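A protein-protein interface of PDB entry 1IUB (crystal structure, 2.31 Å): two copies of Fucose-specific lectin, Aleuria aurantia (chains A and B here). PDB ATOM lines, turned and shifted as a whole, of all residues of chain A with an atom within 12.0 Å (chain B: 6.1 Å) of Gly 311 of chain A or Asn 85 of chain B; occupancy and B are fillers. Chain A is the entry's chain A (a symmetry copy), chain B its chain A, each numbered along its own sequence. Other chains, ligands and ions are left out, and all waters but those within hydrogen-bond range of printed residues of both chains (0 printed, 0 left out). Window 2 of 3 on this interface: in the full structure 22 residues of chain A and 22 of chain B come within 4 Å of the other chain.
Lys 83 of chain B touches Ala 310 of chain A.
Lys 83 of chain B touches Gly 311 of chain A (O to CA, 3.3 Å).
Gly 311 of chain A touches Ser 111 of chain B (O to CB, 3.5 Å).
CE2 of Trp 312 of chain A touches NZ of Lys 58 of chain B (3.4 Å).
Trp 312 of chain A touches Ser 111 of chain B (CH2 to O, 3.2 Å).
Trp 312 of chain A touches Asn 112 of chain B.
The backbone NH (N) of Lys 58 of chain B sits at hydrogen-bond distance from the backbone carbonyl oxygen (O) of Val 81 of chain B (3.0 Å).
The side-chain amino group (NZ) of Lys 58 of chain B lies within hydrogen-bond range of the side-chain amide oxygen (OD1) of Asn 85 of chain B (2.8 Å).
The side-chain amino group of Lys 58 of chain B lies within hydrogen-bond range of the backbone carbonyl oxygen of Ser 111 of chain B (2.9 Å).
The side-chain amide oxygen (OD1) of Asn 82 of chain B lies within hydrogen-bond range of the backbone NH (N) of Asn 85 of chain B (3.3 Å).
O of Asn 85 of chain B is in hydrogen-bond range of N of Val 109 of chain B (2.9 Å).
No position is printed for both chains.
Of the 8 pairs that touch across the chains among the printed residues, none has its exchanged pair printed and touching as well.
NZ of Lys 58 of chain B sits at hydrogen-bond distance from O of Gly 311 of chain A, at 3.0 Å.
The side-chain amide nitrogen (ND2) of Asn 85 of chain B sits at hydrogen-bond distance from the backbone carbonyl oxygen (O) of Gly 311 of chain A (3.0 Å).
Of the 14 printed residues of chain B, 5 touch a printed residue of chain A.
Along chain B the printed residues that touch a printed residue of chain A span positions 58 to 112.
Of the 10 printed residues of chain A, 3 touch a printed residue of chain B.
Printed residues of chain A that touch a printed residue of chain B: Ala 310, Gly 311 and Trp 312.
Hydrophobic or aromatic side chains of chain A within 4 Å of the printed part of chain B: Ala 310 and Trp 312.
Among the printed residues, no Asp or Glu carboxylate lies within 4 Å of a Lys or Arg side-chain nitrogen of the other chain.
Thr 2 of chain A touches none of the printed residues of chain B.
Of chain B, only Lys 58, Lys 83, Asn 85 and Ser 111 come within 4 Å of Gly 311 of chain A.
Printed residues of chain B within 4 Å of Trp 312 of chain A: Lys 58 (3.4 Å), Ser 111 (3.2 Å) and Asn 112 (3.7 Å).
Of the printed residues of chain A, Lys 58 of chain B touches Gly 311 (3.0 Å) and Trp 312 (3.4 Å).
No residue of chain A comes within 4 Å of Val 81 of chain B.
No residue of chain A comes within 4 Å of Asn 82 of chain B.
No residue of chain A comes within 4 Å of Ile 86 of chain B.
No residue of chain A comes within 4 Å of Leu 87 of chain B.
No residue of chain A comes within 4 Å of Lys 108 of chain B.
No residue of chain A comes within 4 Å of Gly 110 of chain B.
Of chain A, only Gly 311 (3.5 Å) and Trp 312 (3.2 Å) come within 4 Å of Ser 111 of chain B.
Of the printed residues of chain A, Asn 112 of chain B touches Trp 312.
The nearest residue of chain A that does not touch Asn 85 of chain B is Trp 312 of chain A (5.0 Å).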
ATOM      1  N   PRO A   1      17.376  13.760  15.076  1.00  0.00           N
ATOM      2  CA  PRO A   1      16.598  13.517  16.301  1.00  0.00           C
ATOM      3  C   PRO A   1      17.114  14.346  17.482  1.00  0.00           C
ATOM      4  O   PRO A   1      18.194  14.934  17.417  1.00  0.00           O
ATOM      5  CB  PRO A   1      16.709  12.026  16.590  1.00  0.00           C
ATOM      6  CG  PRO A   1      18.021  11.682  15.940  1.00  0.00           C
ATOM      7  CD  PRO A   1      18.062  12.520  14.666  1.00  0.00           C
ATOM      8  N   THR A   2      16.345  14.393  18.567  1.00  0.00           N
ATOM      9  CA  THR A   2      16.775  15.139  19.752  1.00  0.00           C
ATOM     10  C   THR A   2      16.541  14.284  20.988  1.00  0.00           C
ATOM     11  O   THR A   2      16.121  13.130  20.886  1.00  0.00           O
ATOM     12  CB  THR A   2      15.958  16.432  19.946  1.00  0.00           C
ATOM     13  OG1 THR A   2      14.610  16.076  20.292  1.00  0.00           O
ATOM     14  CG2 THR A   2      15.951  17.270  18.664  1.00  0.00           C
ATOM     15  N   GLU A   3      16.772  14.883  22.155  1.00  0.00           N
ATOM     16  CA  GLU A   3      16.578  14.197  23.426  1.00  0.00           C
ATOM     17  C   GLU A   3      15.276  14.590  24.107  1.00  0.00           C
ATOM     18  O   GLU A   3      15.040  14.255  25.266  1.00  0.00           O
ATOM     19  CB  GLU A   3      17.760  14.471  24.343  1.00  0.00           C
ATOM     20  CG  GLU A   3      19.064  13.991  23.729  1.00  0.00           C
ATOM     21  CD  GLU A   3      20.277  14.254  24.628  1.00  0.00           C
ATOM     22  OE1 GLU A   3      20.507  15.416  25.044  1.00  0.00           O
ATOM     23  OE2 GLU A   3      21.009  13.294  24.900  1.00  0.00           O
ATOM     24  N   LEU A  30      14.696  11.994  27.251  1.00  0.00           N
ATOM     25  CA  LEU A  30      14.515  10.545  27.109  1.00  0.00           C
ATOM     26  C   LEU A  30      14.820   9.752  28.370  1.00  0.00           C
ATOM     27  O   LEU A  30      14.311   8.642  28.540  1.00  0.00           O
ATOM     28  CB  LEU A  30      15.377  10.014  25.955  1.00  0.00           C
ATOM     29  CG  LEU A  30      15.017  10.593  24.585  1.00  0.00           C
ATOM     30  CD1 LEU A  30      16.014  10.143  23.540  1.00  0.00           C
ATOM     31  CD2 LEU A  30      13.620  10.147  24.225  1.00  0.00           C
ATOM     32  N   GLY A 307      18.800  19.266  22.917  1.00  0.00           N
ATOM     33  CA  GLY A 307      19.849  18.261  22.864  1.00  0.00           C
ATOM     34  C   GLY A 307      19.927  17.390  21.613  1.00  0.00           C
ATOM     35  O   GLY A 307      19.005  17.346  20.786  1.00  0.00           O
ATOM     36  N   THR A 308      21.043  16.677  21.497  1.00  0.00           N
ATOM     37  CA  THR A 308      21.305  15.793  20.379  1.00  0.00           C
ATOM     38  C   THR A 308      21.893  14.507  20.928  1.00  0.00           C
ATOM     39  O   THR A 308      22.887  14.543  21.636  1.00  0.00           O
ATOM     40  CB  THR A 308      22.315  16.434  19.441  1.00  0.00           C
ATOM     41  OG1 THR A 308      21.742  17.626  18.909  1.00  0.00           O
ATOM     42  CG2 THR A 308      22.679  15.498  18.306  1.00  0.00           C
ATOM     43  N   PRO A 309      21.271  13.352  20.638  1.00  0.00           N
ATOM     44  CA  PRO A 309      21.839  12.105  21.167  1.00  0.00           C
ATOM     45  C   PRO A 309      23.182  11.762  20.533  1.00  0.00           C
ATOM     46  O   PRO A 309      23.508  12.196  19.414  1.00  0.00           O
ATOM     47  CB  PRO A 309      20.747  11.065  20.863  1.00  0.00           C
ATOM     48  CG  PRO A 309      20.115  11.587  19.635  1.00  0.00           C
ATOM     49  CD  PRO A 309      20.042  13.093  19.863  1.00  0.00           C
ATOM     50  N   ALA A 310      23.981  11.004  21.268  1.00  0.00           N
ATOM     51  CA  ALA A 310      25.293  10.566  20.788  1.00  0.00           C
ATOM     52  C   ALA A 310      25.086   9.736  19.527  1.00  0.00           C
ATOM     53  O   ALA A 310      24.138   8.961  19.440  1.00  0.00           O
ATOM     54  CB  ALA A 310      25.972   9.708  21.859  1.00  0.00           C
ATOM     55  N   GLY A 311      25.984   9.893  18.565  1.00  0.00           N
ATOM     56  CA  GLY A 311      25.877   9.160  17.319  1.00  0.00           C
ATOM     57  C   GLY A 311      25.199   9.964  16.229  1.00  0.00           C
ATOM     58  O   GLY A 311      25.059   9.496  15.090  1.00  0.00           O
ATOM     59  N   TRP A 312      24.776  11.178  16.571  1.00  0.00           N
ATOM     60  CA  TRP A 312      24.099  12.049  15.624  1.00  0.00           C
ATOM     61  C   TRP A 312      24.711  13.448  15.536  1.00  0.00           C
ATOM     62  O   TRP A 312      24.308  14.205  14.628  1.00  0.00           O
ATOM     63  CB  TRP A 312      22.619  12.170  15.993  1.00  0.00           C
ATOM     64  CG  TRP A 312      21.878  10.893  15.864  1.00  0.00           C
ATOM     65  CD1 TRP A 312      21.756   9.908  16.808  1.00  0.00           C
ATOM     66  CD2 TRP A 312      21.146  10.451  14.715  1.00  0.00           C
ATOM     67  NE1 TRP A 312      20.976   8.875  16.311  1.00  0.00           N
ATOM     68  CE2 TRP A 312      20.595   9.187  15.027  1.00  0.00           C
ATOM     69  CE3 TRP A 312      20.901  11.003  13.447  1.00  0.00           C
ATOM     70  CZ2 TRP A 312      19.806   8.464  14.116  1.00  0.00           C
ATOM     71  CZ3 TRP A 312      20.115  10.286  12.543  1.00  0.00           C
ATOM     72  CH2 TRP A 312      19.577   9.026  12.887  1.00  0.00           C
ATOM     73  OXT TRP A 312      25.570  13.770  16.362  1.00  0.00           O
ATOM     74  N   LYS B  58      22.931   2.841  19.474  1.00  0.00           N
ATOM     75  CA  LYS B  58      22.748   4.271  19.615  1.00  0.00           C
ATOM     76  C   LYS B  58      21.236   4.570  19.543  1.00  0.00           C
ATOM     77  O   LYS B  58      20.453   3.779  19.009  1.00  0.00           O
ATOM     78  CB  LYS B  58      23.474   5.022  18.489  1.00  0.00           C
ATOM     79  CG  LYS B  58      22.707   5.064  17.157  1.00  0.00           C
ATOM     80  CD  LYS B  58      23.299   6.111  16.258  1.00  0.00           C
ATOM     81  CE  LYS B  58      22.733   6.105  14.845  1.00  0.00           C
ATOM     82  NZ  LYS B  58      23.220   7.332  14.068  1.00  0.00           N
ATOM     83  N   VAL B  81      23.613  -0.060  14.877  1.00  0.00           N
ATOM     84  CA  VAL B  81      24.888   0.630  14.973  1.00  0.00           C
ATOM     85  C   VAL B  81      25.105   1.194  16.372  1.00  0.00           C
ATOM     86  O   VAL B  81      24.128   1.470  17.103  1.00  0.00           O
ATOM     87  CB  VAL B  81      25.002   1.773  13.935  1.00  0.00           C
ATOM     88  CG1 VAL B  81      24.268   1.380  12.645  1.00  0.00           C
ATOM     89  CG2 VAL B  81      24.443   3.053  14.502  1.00  0.00           C
ATOM     90  N   ASN B  82      26.373   1.348  16.767  1.00  0.00           N
ATOM     91  CA  ASN B  82      26.655   1.890  18.097  1.00  0.00           C
ATOM     92  C   ASN B  82      26.784   3.400  18.045  1.00  0.00           C
ATOM     93  O   ASN B  82      26.588   4.008  16.980  1.00  0.00           O
ATOM     94  CB  ASN B  82      27.895   1.254  18.781  1.00  0.00           C
ATOM     95  CG  ASN B  82      29.204   1.483  18.030  1.00  0.00           C
ATOM     96  OD1 ASN B  82      29.371   2.455  17.305  1.00  0.00           O
ATOM     97  ND2 ASN B  82      30.156   0.567  18.226  1.00  0.00           N
ATOM     98  N   LYS B  83      27.104   3.999  19.194  1.00  0.00           N
ATOM     99  CA  LYS B  83      27.228   5.454  19.295  1.00  0.00           C
ATOM    100  C   LYS B  83      28.312   6.053  18.432  1.00  0.00           C
ATOM    101  O   LYS B  83      28.353   7.272  18.280  1.00  0.00           O
ATOM    102  CB  LYS B  83      27.419   5.866  20.747  1.00  0.00           C
ATOM    103  CG  LYS B  83      26.257   5.461  21.591  1.00  0.00           C
ATOM    104  CD  LYS B  83      26.418   5.936  23.023  1.00  0.00           C
ATOM    105  CE  LYS B  83      25.344   5.298  23.920  1.00  0.00           C
ATOM    106  NZ  LYS B  83      25.417   5.895  25.268  1.00  0.00           N
ATOM    107  N   ASP B  84      29.182   5.221  17.855  1.00  0.00           N
ATOM    108  CA  ASP B  84      30.223   5.741  16.964  1.00  0.00           C
ATOM    109  C   ASP B  84      29.860   5.404  15.527  1.00  0.00           C
ATOM    110  O   ASP B  84      30.676   5.531  14.607  1.00  0.00           O
ATOM    111  CB  ASP B  84      31.596   5.155  17.325  1.00  0.00           C
ATOM    112  CG  ASP B  84      31.966   5.427  18.773  1.00  0.00           C
ATOM    113  OD1 ASP B  84      31.834   4.526  19.622  1.00  0.00           O
ATOM    114  OD2 ASP B  84      32.347   6.566  19.067  1.00  0.00           O
ATOM    115  N   ASN B  85      28.613   4.979  15.343  1.00  0.00           N
ATOM    116  CA  ASN B  85      28.104   4.611  14.024  1.00  0.00           C
ATOM    117  C   ASN B  85      28.809   3.447  13.372  1.00  0.00           C
ATOM    118  O   ASN B  85      28.982   3.414  12.149  1.00  0.00           O
ATOM    119  CB  ASN B  85      28.096   5.827  13.090  1.00  0.00           C
ATOM    120  CG  ASN B  85      26.941   6.767  13.412  1.00  0.00           C
ATOM    121  OD1 ASN B  85      25.790   6.327  13.500  1.00  0.00           O
ATOM    122  ND2 ASN B  85      27.235   8.041  13.612  1.00  0.00           N
ATOM    123  N   ILE B  86      29.203   2.481  14.200  1.00  0.00           N
ATOM    124  CA  ILE B  86      29.858   1.288  13.688  1.00  0.00           C
ATOM    125  C   ILE B  86      28.799   0.197  13.601  1.00  0.00           C
ATOM    126  O   ILE B  86      28.107  -0.095  14.579  1.00  0.00           O
ATOM    127  CB  ILE B  86      31.002   0.804  14.608  1.00  0.00           C
ATOM    128  CG1 ILE B  86      32.080   1.885  14.696  1.00  0.00           C
ATOM    129  CG2 ILE B  86      31.612  -0.490  14.039  1.00  0.00           C
ATOM    130  CD1 ILE B  86      33.072   1.663  15.831  1.00  0.00           C
ATOM    131  N   LEU B  87      28.675  -0.380  12.412  1.00  0.00           N
ATOM    132  CA  LEU B  87      27.723  -1.448  12.143  1.00  0.00           C
ATOM    133  C   LEU B  87      28.057  -2.624  13.049  1.00  0.00           C
ATOM    134  O   LEU B  87      29.201  -3.091  13.070  1.00  0.00           O
ATOM    135  CB  LEU B  87      27.816  -1.835  10.662  1.00  0.00           C
ATOM    136  CG  LEU B  87      26.779  -2.777  10.091  1.00  0.00           C
ATOM    137  CD1 LEU B  87      25.413  -2.456  10.651  1.00  0.00           C
ATOM    138  CD2 LEU B  87      26.794  -2.653   8.570  1.00  0.00           C
ATOM    139  N   VAL B 107      32.999  -1.403  10.191  1.00  0.00           N
ATOM    140  CA  VAL B 107      32.308  -0.701   9.109  1.00  0.00           C
ATOM    141  C   VAL B 107      31.561   0.533   9.665  1.00  0.00           C
ATOM    142  O   VAL B 107      30.745   0.425  10.598  1.00  0.00           O
ATOM    143  CB  VAL B 107      31.305  -1.634   8.380  1.00  0.00           C
ATOM    144  CG1 VAL B 107      30.539  -0.842   7.330  1.00  0.00           C
ATOM    145  CG2 VAL B 107      32.065  -2.789   7.711  1.00  0.00           C
ATOM    146  N   LYS B 108      31.836   1.698   9.085  1.00  0.00           N
ATOM    147  CA  LYS B 108      31.211   2.936   9.530  1.00  0.00           C
ATOM    148  C   LYS B 108      30.039   3.332   8.641  1.00  0.00           C
ATOM    149  O   LYS B 108      30.167   3.411   7.430  1.00  0.00           O
ATOM    150  CB  LYS B 108      32.231   4.087   9.572  1.00  0.00           C
ATOM    151  CG  LYS B 108      31.715   5.297  10.367  1.00  0.00           C
ATOM    152  CD  LYS B 108      32.590   6.538  10.215  1.00  0.00           C
ATOM    153  CE  LYS B 108      31.851   7.801  10.714  1.00  0.00           C
ATOM    154  NZ  LYS B 108      30.506   8.025  10.037  1.00  0.00           N
ATOM    155  N   VAL B 109      28.905   3.609   9.270  1.00  0.00           N
ATOM    156  CA  VAL B 109      27.670   3.958   8.568  1.00  0.00           C
ATOM    157  C   VAL B 109      27.328   5.448   8.660  1.00  0.00           C
ATOM    158  O   VAL B 109      27.696   6.100   9.632  1.00  0.00           O
ATOM    159  CB  VAL B 109      26.517   3.124   9.189  1.00  0.00           C
ATOM    160  CG1 VAL B 109      25.208   3.569   8.667  1.00  0.00           C
ATOM    161  CG2 VAL B 109      26.748   1.643   8.907  1.00  0.00           C
ATOM    162  N   GLY B 110      26.657   5.995   7.648  1.00  0.00           N
ATOM    163  CA  GLY B 110      26.241   7.394   7.718  1.00  0.00           C
ATOM    164  C   GLY B 110      25.286   7.478   8.915  1.00  0.00           C
ATOM    165  O   GLY B 110      24.487   6.565   9.123  1.00  0.00           O
ATOM    166  N   SER B 111      25.327   8.552   9.701  1.00  0.00           N
ATOM    167  CA  SER B 111      24.457   8.611  10.881  1.00  0.00           C
ATOM    168  C   SER B 111      22.958   8.476  10.605  1.00  0.00           C
ATOM    169  O   SER B 111      22.224   7.936  11.443  1.00  0.00           O
ATOM    170  CB  SER B 111      24.696   9.894  11.655  1.00  0.00           C
ATOM    171  OG  SER B 111      24.228  10.977  10.908  1.00  0.00           O
ATOM    172  N   ASN B 112      22.498   8.965   9.449  1.00  0.00           N
ATOM    173  CA  ASN B 112      21.073   8.869   9.100  1.00  0.00           C
ATOM    174  C   ASN B 112      20.760   7.668   8.190  1.00  0.00           C
ATOM    175  O   ASN B 112      19.661   7.542   7.646  1.00  0.00           O
ATOM    176  CB  ASN B 112      20.578  10.174   8.434  1.00  0.00           C
ATOM    177  CG  ASN B 112      19.040  10.253   8.356  1.00  0.00           C
ATOM    178  OD1 ASN B 112      18.331   9.876   9.292  1.00  0.00           O
ATOM    179  ND2 ASN B 112      18.531  10.746   7.238  1.00  0.00           N
